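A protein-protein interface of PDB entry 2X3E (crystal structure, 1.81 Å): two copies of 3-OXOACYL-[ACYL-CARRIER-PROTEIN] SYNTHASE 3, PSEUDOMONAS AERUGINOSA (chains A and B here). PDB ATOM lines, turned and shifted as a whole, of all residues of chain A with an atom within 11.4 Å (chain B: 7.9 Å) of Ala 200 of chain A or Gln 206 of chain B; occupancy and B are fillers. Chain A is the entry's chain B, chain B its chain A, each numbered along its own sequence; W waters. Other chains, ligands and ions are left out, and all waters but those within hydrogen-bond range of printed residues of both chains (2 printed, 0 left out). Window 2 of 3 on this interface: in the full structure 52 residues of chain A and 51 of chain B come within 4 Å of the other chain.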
ATOM      1  N   PRO A 195       8.459   2.355 -18.412  1.00  0.00           N
ATOM      2  CA  PRO A 195       7.879   3.484 -17.679  1.00  0.00           C
ATOM      3  C   PRO A 195       7.499   3.134 -16.244  1.00  0.00           C
ATOM      4  O   PRO A 195       7.237   1.965 -15.939  1.00  0.00           O
ATOM      5  CB  PRO A 195       6.619   3.830 -18.485  1.00  0.00           C
ATOM      6  CG  PRO A 195       6.779   3.142 -19.809  1.00  0.00           C
ATOM      7  CD  PRO A 195       7.632   1.950 -19.562  1.00  0.00           C
ATOM      8  N   ALA A 196       7.490   4.139 -15.373  1.00  0.00           N
ATOM      9  CA  ALA A 196       6.838   4.020 -14.072  1.00  0.00           C
ATOM     10  C   ALA A 196       5.335   4.115 -14.327  1.00  0.00           C
ATOM     11  O   ALA A 196       4.907   4.894 -15.169  1.00  0.00           O
ATOM     12  CB  ALA A 196       7.300   5.133 -13.133  1.00  0.00           C
ATOM     13  N   VAL A 197       4.534   3.324 -13.620  1.00  0.00           N
ATOM     14  CA  VAL A 197       3.096   3.282 -13.889  1.00  0.00           C
ATOM     15  C   VAL A 197       2.353   4.368 -13.108  1.00  0.00           C
ATOM     16  O   VAL A 197       2.582   4.550 -11.911  1.00  0.00           O
ATOM     17  CB  VAL A 197       2.486   1.900 -13.569  1.00  0.00           C
ATOM     18  CG1 VAL A 197       0.989   1.875 -13.916  1.00  0.00           C
ATOM     19  CG2 VAL A 197       3.236   0.806 -14.318  1.00  0.00           C
ATOM     20  N   SER A 198       1.476   5.089 -13.798  1.00  0.00           N
ATOM     21  CA  SER A 198       0.706   6.174 -13.193  1.00  0.00           C
ATOM     22  C   SER A 198      -0.289   5.626 -12.182  1.00  0.00           C
ATOM     23  O   SER A 198      -0.896   4.579 -12.408  1.00  0.00           O
ATOM     24  CB  SER A 198      -0.046   6.966 -14.270  1.00  0.00           C
ATOM     25  OG  SER A 198      -0.963   7.889 -13.691  1.00  0.00           O
ATOM     26  N   ARG A 199      -0.457   6.345 -11.073  1.00  0.00           N
ATOM     27  CA  ARG A 199      -1.436   5.959 -10.050  1.00  0.00           C
ATOM     28  C   ARG A 199      -2.792   6.648 -10.203  1.00  0.00           C
ATOM     29  O   ARG A 199      -3.684   6.440  -9.377  1.00  0.00           O
ATOM     30  CB  ARG A 199      -0.867   6.226  -8.657  1.00  0.00           C
ATOM     31  CG  ARG A 199       0.351   5.378  -8.334  1.00  0.00           C
ATOM     32  CD  ARG A 199       1.210   6.044  -7.283  1.00  0.00           C
ATOM     33  NE  ARG A 199       2.225   5.151  -6.725  1.00  0.00           N
ATOM     34  CZ  ARG A 199       3.524   5.171  -7.017  1.00  0.00           C
ATOM     35  NH1 ARG A 199       4.032   6.046  -7.887  1.00  0.00           N
ATOM     36  NH2 ARG A 199       4.332   4.300  -6.426  1.00  0.00           N
ATOM     37  N   ALA A 200      -2.957   7.461 -11.246  1.00  0.00           N
ATOM     38  CA  ALA A 200      -4.235   8.148 -11.489  1.00  0.00           C
ATOM     39  C   ALA A 200      -5.252   7.202 -12.124  1.00  0.00           C
ATOM     40  O   ALA A 200      -4.881   6.260 -12.828  1.00  0.00           O
ATOM     41  CB  ALA A 200      -4.030   9.374 -12.371  1.00  0.00           C
ATOM     42  N   ASN A 209       2.221   0.116 -20.265  1.00  0.00           N
ATOM     43  CA  ASN A 209       3.515   0.619 -19.825  1.00  0.00           C
ATOM     44  C   ASN A 209       4.535  -0.504 -19.666  1.00  0.00           C
ATOM     45  O   ASN A 209       5.157  -0.655 -18.612  1.00  0.00           O
ATOM     46  CB  ASN A 209       3.370   1.384 -18.504  1.00  0.00           C
ATOM     47  CG  ASN A 209       2.470   2.587 -18.628  1.00  0.00           C
ATOM     48  OD1 ASN A 209       2.726   3.487 -19.431  1.00  0.00           O
ATOM     49  ND2 ASN A 209       1.406   2.615 -17.832  1.00  0.00           N
ATOM     50  N   TYR A 210       4.703  -1.294 -20.719  1.00  0.00           N
ATOM     51  CA  TYR A 210       5.705  -2.354 -20.712  1.00  0.00           C
ATOM     52  C   TYR A 210       7.061  -1.796 -21.133  1.00  0.00           C
ATOM     53  O   TYR A 210       7.155  -0.655 -21.597  1.00  0.00           O
ATOM     54  CB  TYR A 210       5.298  -3.475 -21.660  1.00  0.00           C
ATOM     55  CG  TYR A 210       4.016  -4.164 -21.263  1.00  0.00           C
ATOM     56  CD1 TYR A 210       2.851  -3.986 -21.999  1.00  0.00           C
ATOM     57  CD2 TYR A 210       3.971  -4.994 -20.144  1.00  0.00           C
ATOM     58  CE1 TYR A 210       1.669  -4.623 -21.637  1.00  0.00           C
ATOM     59  CE2 TYR A 210       2.797  -5.636 -19.774  1.00  0.00           C
ATOM     60  CZ  TYR A 210       1.652  -5.444 -20.522  1.00  0.00           C
ATOM     61  OH  TYR A 210       0.492  -6.079 -20.160  1.00  0.00           O
ATOM     62  N   HIS B 144       3.702  11.710  -5.088  1.00  0.00           N
ATOM     63  CA  HIS B 144       3.139  10.902  -6.180  1.00  0.00           C
ATOM     64  C   HIS B 144       2.756   9.501  -5.717  1.00  0.00           C
ATOM     65  O   HIS B 144       1.931   8.850  -6.351  1.00  0.00           O
ATOM     66  CB  HIS B 144       4.117  10.776  -7.353  1.00  0.00           C
ATOM     67  CG  HIS B 144       4.387  12.067  -8.057  1.00  0.00           C
ATOM     68  ND1 HIS B 144       5.641  12.417  -8.507  1.00  0.00           N
ATOM     69  CD2 HIS B 144       3.568  13.093  -8.388  1.00  0.00           C
ATOM     70  CE1 HIS B 144       5.584  13.602  -9.086  1.00  0.00           C
ATOM     71  NE2 HIS B 144       4.338  14.036  -9.026  1.00  0.00           N
ATOM     72  N   VAL B 197       4.966  -2.157  -8.744  1.00  0.00           N
ATOM     73  CA  VAL B 197       3.753  -2.385  -9.526  1.00  0.00           C
ATOM     74  C   VAL B 197       3.633  -3.867  -9.905  1.00  0.00           C
ATOM     75  O   VAL B 197       4.627  -4.502 -10.255  1.00  0.00           O
ATOM     76  CB  VAL B 197       3.748  -1.512 -10.811  1.00  0.00           C
ATOM     77  CG1 VAL B 197       4.897  -1.897 -11.742  1.00  0.00           C
ATOM     78  CG2 VAL B 197       2.427  -1.637 -11.538  1.00  0.00           C
ATOM     79  N   SER B 198       2.426  -4.416  -9.808  1.00  0.00           N
ATOM     80  CA  SER B 198       2.157  -5.787 -10.257  1.00  0.00           C
ATOM     81  C   SER B 198       2.042  -5.824 -11.775  1.00  0.00           C
ATOM     82  O   SER B 198       1.804  -4.797 -12.408  1.00  0.00           O
ATOM     83  CB  SER B 198       0.867  -6.319  -9.640  1.00  0.00           C
ATOM     84  OG  SER B 198       0.655  -7.672 -10.016  1.00  0.00           O
ATOM     85  N   ARG B 199       2.201  -7.012 -12.351  1.00  0.00           N
ATOM     86  CA  ARG B 199       2.111  -7.183 -13.801  1.00  0.00           C
ATOM     87  C   ARG B 199       0.716  -6.822 -14.306  1.00  0.00           C
ATOM     88  O   ARG B 199       0.571  -6.265 -15.396  1.00  0.00           O
ATOM     89  CB  ARG B 199       2.485  -8.617 -14.203  1.00  0.00           C
ATOM     90  CG  ARG B 199       3.941  -8.968 -13.879  1.00  0.00           C
ATOM     91  CD  ARG B 199       4.315 -10.373 -14.321  1.00  0.00           C
ATOM     92  NE  ARG B 199       3.662 -11.401 -13.509  1.00  0.00           N
ATOM     93  CZ  ARG B 199       4.072 -11.812 -12.307  1.00  0.00           C
ATOM     94  NH1 ARG B 199       5.152 -11.292 -11.729  1.00  0.00           N
ATOM     95  NH2 ARG B 199       3.388 -12.758 -11.673  1.00  0.00           N
ATOM     96  N   ALA B 200      -0.303  -7.135 -13.506  1.00  0.00           N
ATOM     97  CA  ALA B 200      -1.680  -6.739 -13.806  1.00  0.00           C
ATOM     98  C   ALA B 200      -1.835  -5.214 -13.856  1.00  0.00           C
ATOM     99  O   ALA B 200      -2.498  -4.685 -14.747  1.00  0.00           O
ATOM    100  CB  ALA B 200      -2.641  -7.339 -12.780  1.00  0.00           C
ATOM    101  N   GLU B 201      -1.222  -4.513 -12.904  1.00  0.00           N
ATOM    102  CA  GLU B 201      -1.252  -3.047 -12.890  1.00  0.00           C
ATOM    103  C   GLU B 201      -0.503  -2.450 -14.082  1.00  0.00           C
ATOM    104  O   GLU B 201      -0.931  -1.442 -14.645  1.00  0.00           O
ATOM    105  CB  GLU B 201      -0.657  -2.505 -11.594  1.00  0.00           C
ATOM    106  CG  GLU B 201      -1.549  -2.652 -10.377  1.00  0.00           C
ATOM    107  CD  GLU B 201      -0.853  -2.205  -9.098  1.00  0.00           C
ATOM    108  OE1 GLU B 201       0.371  -2.429  -8.967  1.00  0.00           O
ATOM    109  OE2 GLU B 201      -1.539  -1.632  -8.221  1.00  0.00           O
ATOM    110  N   ARG B 202       0.609  -3.072 -14.468  1.00  0.00           N
ATOM    111  CA  ARG B 202       1.385  -2.599 -15.616  1.00  0.00           C
ATOM    112  C   ARG B 202       0.575  -2.747 -16.902  1.00  0.00           C
ATOM    113  O   ARG B 202       0.632  -1.888 -17.783  1.00  0.00           O
ATOM    114  CB  ARG B 202       2.719  -3.348 -15.726  1.00  0.00           C
ATOM    115  CG  ARG B 202       3.678  -2.751 -16.747  1.00  0.00           C
ATOM    116  CD  ARG B 202       5.080  -3.352 -16.648  1.00  0.00           C
ATOM    117  NE  ARG B 202       5.804  -2.900 -15.461  1.00  0.00           N
ATOM    118  CZ  ARG B 202       6.357  -1.693 -15.320  1.00  0.00           C
ATOM    119  NH1 ARG B 202       6.277  -0.782 -16.288  1.00  0.00           N
ATOM    120  NH2 ARG B 202       6.994  -1.388 -14.197  1.00  0.00           N
ATOM    121  N   SER B 203      -0.186  -3.836 -16.989  1.00  0.00           N
ATOM    122  CA  SER B 203      -1.067  -4.093 -18.128  1.00  0.00           C
ATOM    123  C   SER B 203      -2.217  -3.090 -18.203  1.00  0.00           C
ATOM    124  O   SER B 203      -2.582  -2.630 -19.288  1.00  0.00           O
ATOM    125  CB  SER B 203      -1.643  -5.507 -18.040  1.00  0.00           C
ATOM    126  OG  SER B 203      -2.373  -5.830 -19.211  1.00  0.00           O
ATOM    127  N   SER B 204      -2.790  -2.767 -17.045  1.00  0.00           N
ATOM    128  CA  SER B 204      -3.917  -1.840 -16.966  1.00  0.00           C
ATOM    129  C   SER B 204      -3.504  -0.394 -17.239  1.00  0.00           C
ATOM    130  O   SER B 204      -4.315   0.414 -17.695  1.00  0.00           O
ATOM    131  CB  SER B 204      -4.570  -1.929 -15.584  1.00  0.00           C
ATOM    132  OG  SER B 204      -5.788  -1.203 -15.549  1.00  0.00           O
ATOM    133  N   GLY B 205      -2.243  -0.073 -16.956  1.00  0.00           N
ATOM    134  CA  GLY B 205      -1.772   1.307 -17.007  1.00  0.00           C
ATOM    135  C   GLY B 205      -2.219   2.097 -15.789  1.00  0.00           C
ATOM    136  O   GLY B 205      -2.219   3.329 -15.806  1.00  0.00           O
ATOM    137  N   GLN B 206      -2.602   1.377 -14.734  1.00  0.00           N
ATOM    138  CA  GLN B 206      -3.022   1.978 -13.475  1.00  0.00           C
ATOM    139  C   GLN B 206      -2.451   1.156 -12.332  1.00  0.00           C
ATOM    140  O   GLN B 206      -2.625  -0.067 -12.291  1.00  0.00           O
ATOM    141  CB  GLN B 206      -4.549   2.010 -13.370  1.00  0.00           C
ATOM    142  CG  GLN B 206      -5.097   3.071 -12.410  1.00  0.00           C
ATOM    143  CD  GLN B 206      -4.808   2.798 -10.935  1.00  0.00           C
ATOM    144  OE1 GLN B 206      -4.433   3.706 -10.194  1.00  0.00           O
ATOM    145  NE2 GLN B 206      -4.994   1.553 -10.502  1.00  0.00           N
ATOM    146  N   ALA B 207      -1.783   1.835 -11.406  1.00  0.00           N
ATOM    147  CA  ALA B 207      -1.246   1.190 -10.214  1.00  0.00           C
ATOM    148  C   ALA B 207      -1.839   1.820  -8.958  1.00  0.00           C
ATOM    149  O   ALA B 207      -2.194   2.999  -8.955  1.00  0.00           O
ATOM    150  CB  ALA B 207       0.271   1.297 -10.201  1.00  0.00           C
ATOM    151  N   SER B 208      -1.960   1.019  -7.901  1.00  0.00           N
ATOM    152  CA  SER B 208      -2.363   1.505  -6.580  1.00  0.00           C
ATOM    153  C   SER B 208      -1.290   1.134  -5.551  1.00  0.00           C
ATOM    154  O   SER B 208      -1.601   0.797  -4.405  1.00  0.00           O
ATOM    155  CB  SER B 208      -3.717   0.910  -6.181  1.00  0.00           C
ATOM    156  OG  SER B 208      -4.701   1.178  -7.166  1.00  0.00           O
ATOM    157  N   ASN B 209      -0.024   1.205  -5.969  1.00  0.00           N
ATOM    158  CA  ASN B 209       1.101   0.867  -5.095  1.00  0.00           C
ATOM    159  C   ASN B 209       1.511   2.078  -4.250  1.00  0.00           C
ATOM    160  O   ASN B 209       2.350   2.890  -4.660  1.00  0.00           O
ATOM    161  CB  ASN B 209       2.283   0.290  -5.898  1.00  0.00           C
ATOM    162  CG  ASN B 209       2.822   1.249  -6.959  1.00  0.00           C
ATOM    163  OD1 ASN B 209       2.061   1.843  -7.724  1.00  0.00           O
ATOM    164  ND2 ASN B 209       4.145   1.380  -7.020  1.00  0.00           N
ATOM    165  N   TYR B 210       0.887   2.201  -3.081  1.00  0.00           N
ATOM    166  CA  TYR B 210       1.063   3.369  -2.226  1.00  0.00           C
ATOM    167  C   TYR B 210       2.083   3.124  -1.123  1.00  0.00           C
ATOM    168  O   TYR B 210       2.239   1.999  -0.636  1.00  0.00           O
ATOM    169  CB  TYR B 210      -0.263   3.773  -1.572  1.00  0.00           C
ATOM    170  CG  TYR B 210      -1.372   4.168  -2.529  1.00  0.00           C
ATOM    171  CD1 TYR B 210      -2.663   3.679  -2.360  1.00  0.00           C
ATOM    172  CD2 TYR B 210      -1.134   5.036  -3.595  1.00  0.00           C
ATOM    173  CE1 TYR B 210      -3.694   4.038  -3.226  1.00  0.00           C
ATOM    174  CE2 TYR B 210      -2.158   5.401  -4.468  1.00  0.00           C
ATOM    175  CZ  TYR B 210      -3.436   4.896  -4.276  1.00  0.00           C
ATOM    176  OH  TYR B 210      -4.458   5.249  -5.129  1.00  0.00           O
HETATM  177  O   HOH W   1       3.479   3.292  -9.708  1.00  0.00           O
HETATM  178  O   HOH W   2      -3.555   5.571 -15.204  1.00  0.00           O
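The backbone carbonyl oxygen (O) of Ser 198 of chain A lies within hydrogen-bond range of the backbone NH (N) of Ala 207 of chain B, at 3.1 Å.
The backbone carbonyl oxygen of Pro 195 of chain A sits at hydrogen-bond distance from the guanidinium group of Arg 202 of chain B, at 2.9 Å.
OE1 of Gln 206 of chain B sits close to O of Arg 199 of chain A.
The side-chain hydroxyl (OG) of Ser 203 of chain B is in hydrogen-bond range of the side-chain hydroxyl (OH) of Tyr 210 of chain A (3.0 Å).
The backbone carbonyl oxygen (O) of Asn 209 of chain A is in hydrogen-bond range of the guanidinium group (NH1) of Arg 202 of chain B (2.6 Å).
NH2 of Arg 199 of chain A sits close to ND2 of Asn 209 of chain B (3.0 Å).
NE2 of Gln 206 of chain B sits at hydrogen-bond distance from OG of Ser 208 of chain B, at 3.4 Å.
The backbone carbonyl oxygen (O) of Glu 201 of chain B is in hydrogen-bond range of the backbone NH (N) of Gln 206 of chain B, 3.3 Å away.
The backbone NH (N) of Ser 198 of chain B is in hydrogen-bond range of the side-chain carboxylate (OE1) of Glu 201 of chain B (3.0 Å).
The side-chain hydroxyl (OG) of Ser 198 of chain A lies within hydrogen-bond range of the backbone NH (N) of Ala 200 of chain A (3.2 Å).
The side-chain carboxylate of Glu 201 of chain B lies within hydrogen-bond range of the backbone NH of Ser 208 of chain B, 2.7 Å away.
Among the printed residues, merely in contact across the chains: Arg 199 of chain A with His 144 of chain B (3.0 Å), Ala 200 of chain A with Gln 206 of chain B (3.2 Å), Arg 199 of chain A with Ala 207 of chain B (3.2 Å), Ser 198 of chain A with Gln 206 of chain B (3.5 Å), Asn 209 of chain A with Gly 205 of chain B (3.5 Å), Val 197 of chain A with Gln 206 of chain B (3.7 Å), Val 197 of chain A with Gly 205 of chain B (3.7 Å), Val 197 of chain A with Ala 207 of chain B (3.7 Å), Val 197 of chain A with Val 197 of chain B (3.8 Å), Ser 198 of chain A with Gly 205 of chain B (3.9 Å), Val 197 of chain A with Glu 201 of chain B (3.9 Å) and Val 197 of chain A with Arg 202 of chain B (3.96 Å).
Of the printed residues of chain B, Pro 195 of chain A touches Arg 202 (2.9 Å).
Of chain B, only Gln 206 comes within 4 Å of Ala 200 of chain A.
Of chain A, only Val 197 comes within 4 Å of Glu 201 of chain B.
No residue of chain A comes within 4 Å of Ser 204 of chain B.
Gly 205 of chain B touches three residues of chain A.
Of chain A, only Val 197 (3.7 Å), Ser 198 (3.5 Å), Arg 199 (3.0 Å) and Ala 200 (3.2 Å) come within 4 Å of Gln 206 of chain B.
Ser 208 of chain B touches none of the printed residues of chain A.
Of the printed residues of chain A, Asn 209 of chain B touches Arg 199.
Tyr 210 of chain B touches none of the printed residues of chain A.
The nearest residue of chain A that does not touch Gln 206 of chain B is Asn 209 of chain A (5.2 Å).
Of the 15 printed residues of chain B, 9 touch a printed residue of chain A.
Printed residues of chain B that touch a printed residue of chain A: His 144, Val 197, Glu 201, Arg 202, Ser 203, Gly 205, Gln 206, Ala 207 and Asn 209.
Hydrophobic or aromatic side chains of chain B within 4 Å of the printed part of chain A: Val 197 and Ala 207.
Along chain B the printed residues that touch a printed residue of chain A span positions 144 to 209.
Of the 8 printed residues of chain A, 7 touch a printed residue of chain B.
Printed residues of chain A that touch a printed residue of chain B: Pro 195, Val 197, Ser 198, Arg 199, Ala 200, Asn 209 and Tyr 210.
Hydrophobic or aromatic side chains of chain A that line the printed part of chain B: Val 197 and Tyr 210.
Among the printed residues, 18 pairs touch across the chains.
Val 197 of chain A touches its own counterpart, Val 197 of chain B.
Arg 199 of chain A touches Asn 209 of chain B, but with the chains exchanged Asn 209 of chain A does not touch Arg 199 of chain B (7.9 Å).
Of the 18 pairs that touch across the chains among the printed residues, 1 has its exchanged pair printed and touching as well.
Water W2 lies within hydrogen-bond range of O of Gly 205 of chain B (2.7 Å) and O of Ala 200 of chain A (2.8 Å).
Water W1 lies within hydrogen-bond range of O of Val 197 of chain A (2.7 Å), OD1 of Asn 209 of chain B (2.8 Å) and NH1 of Arg 199 of chain A (3.3 Å).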
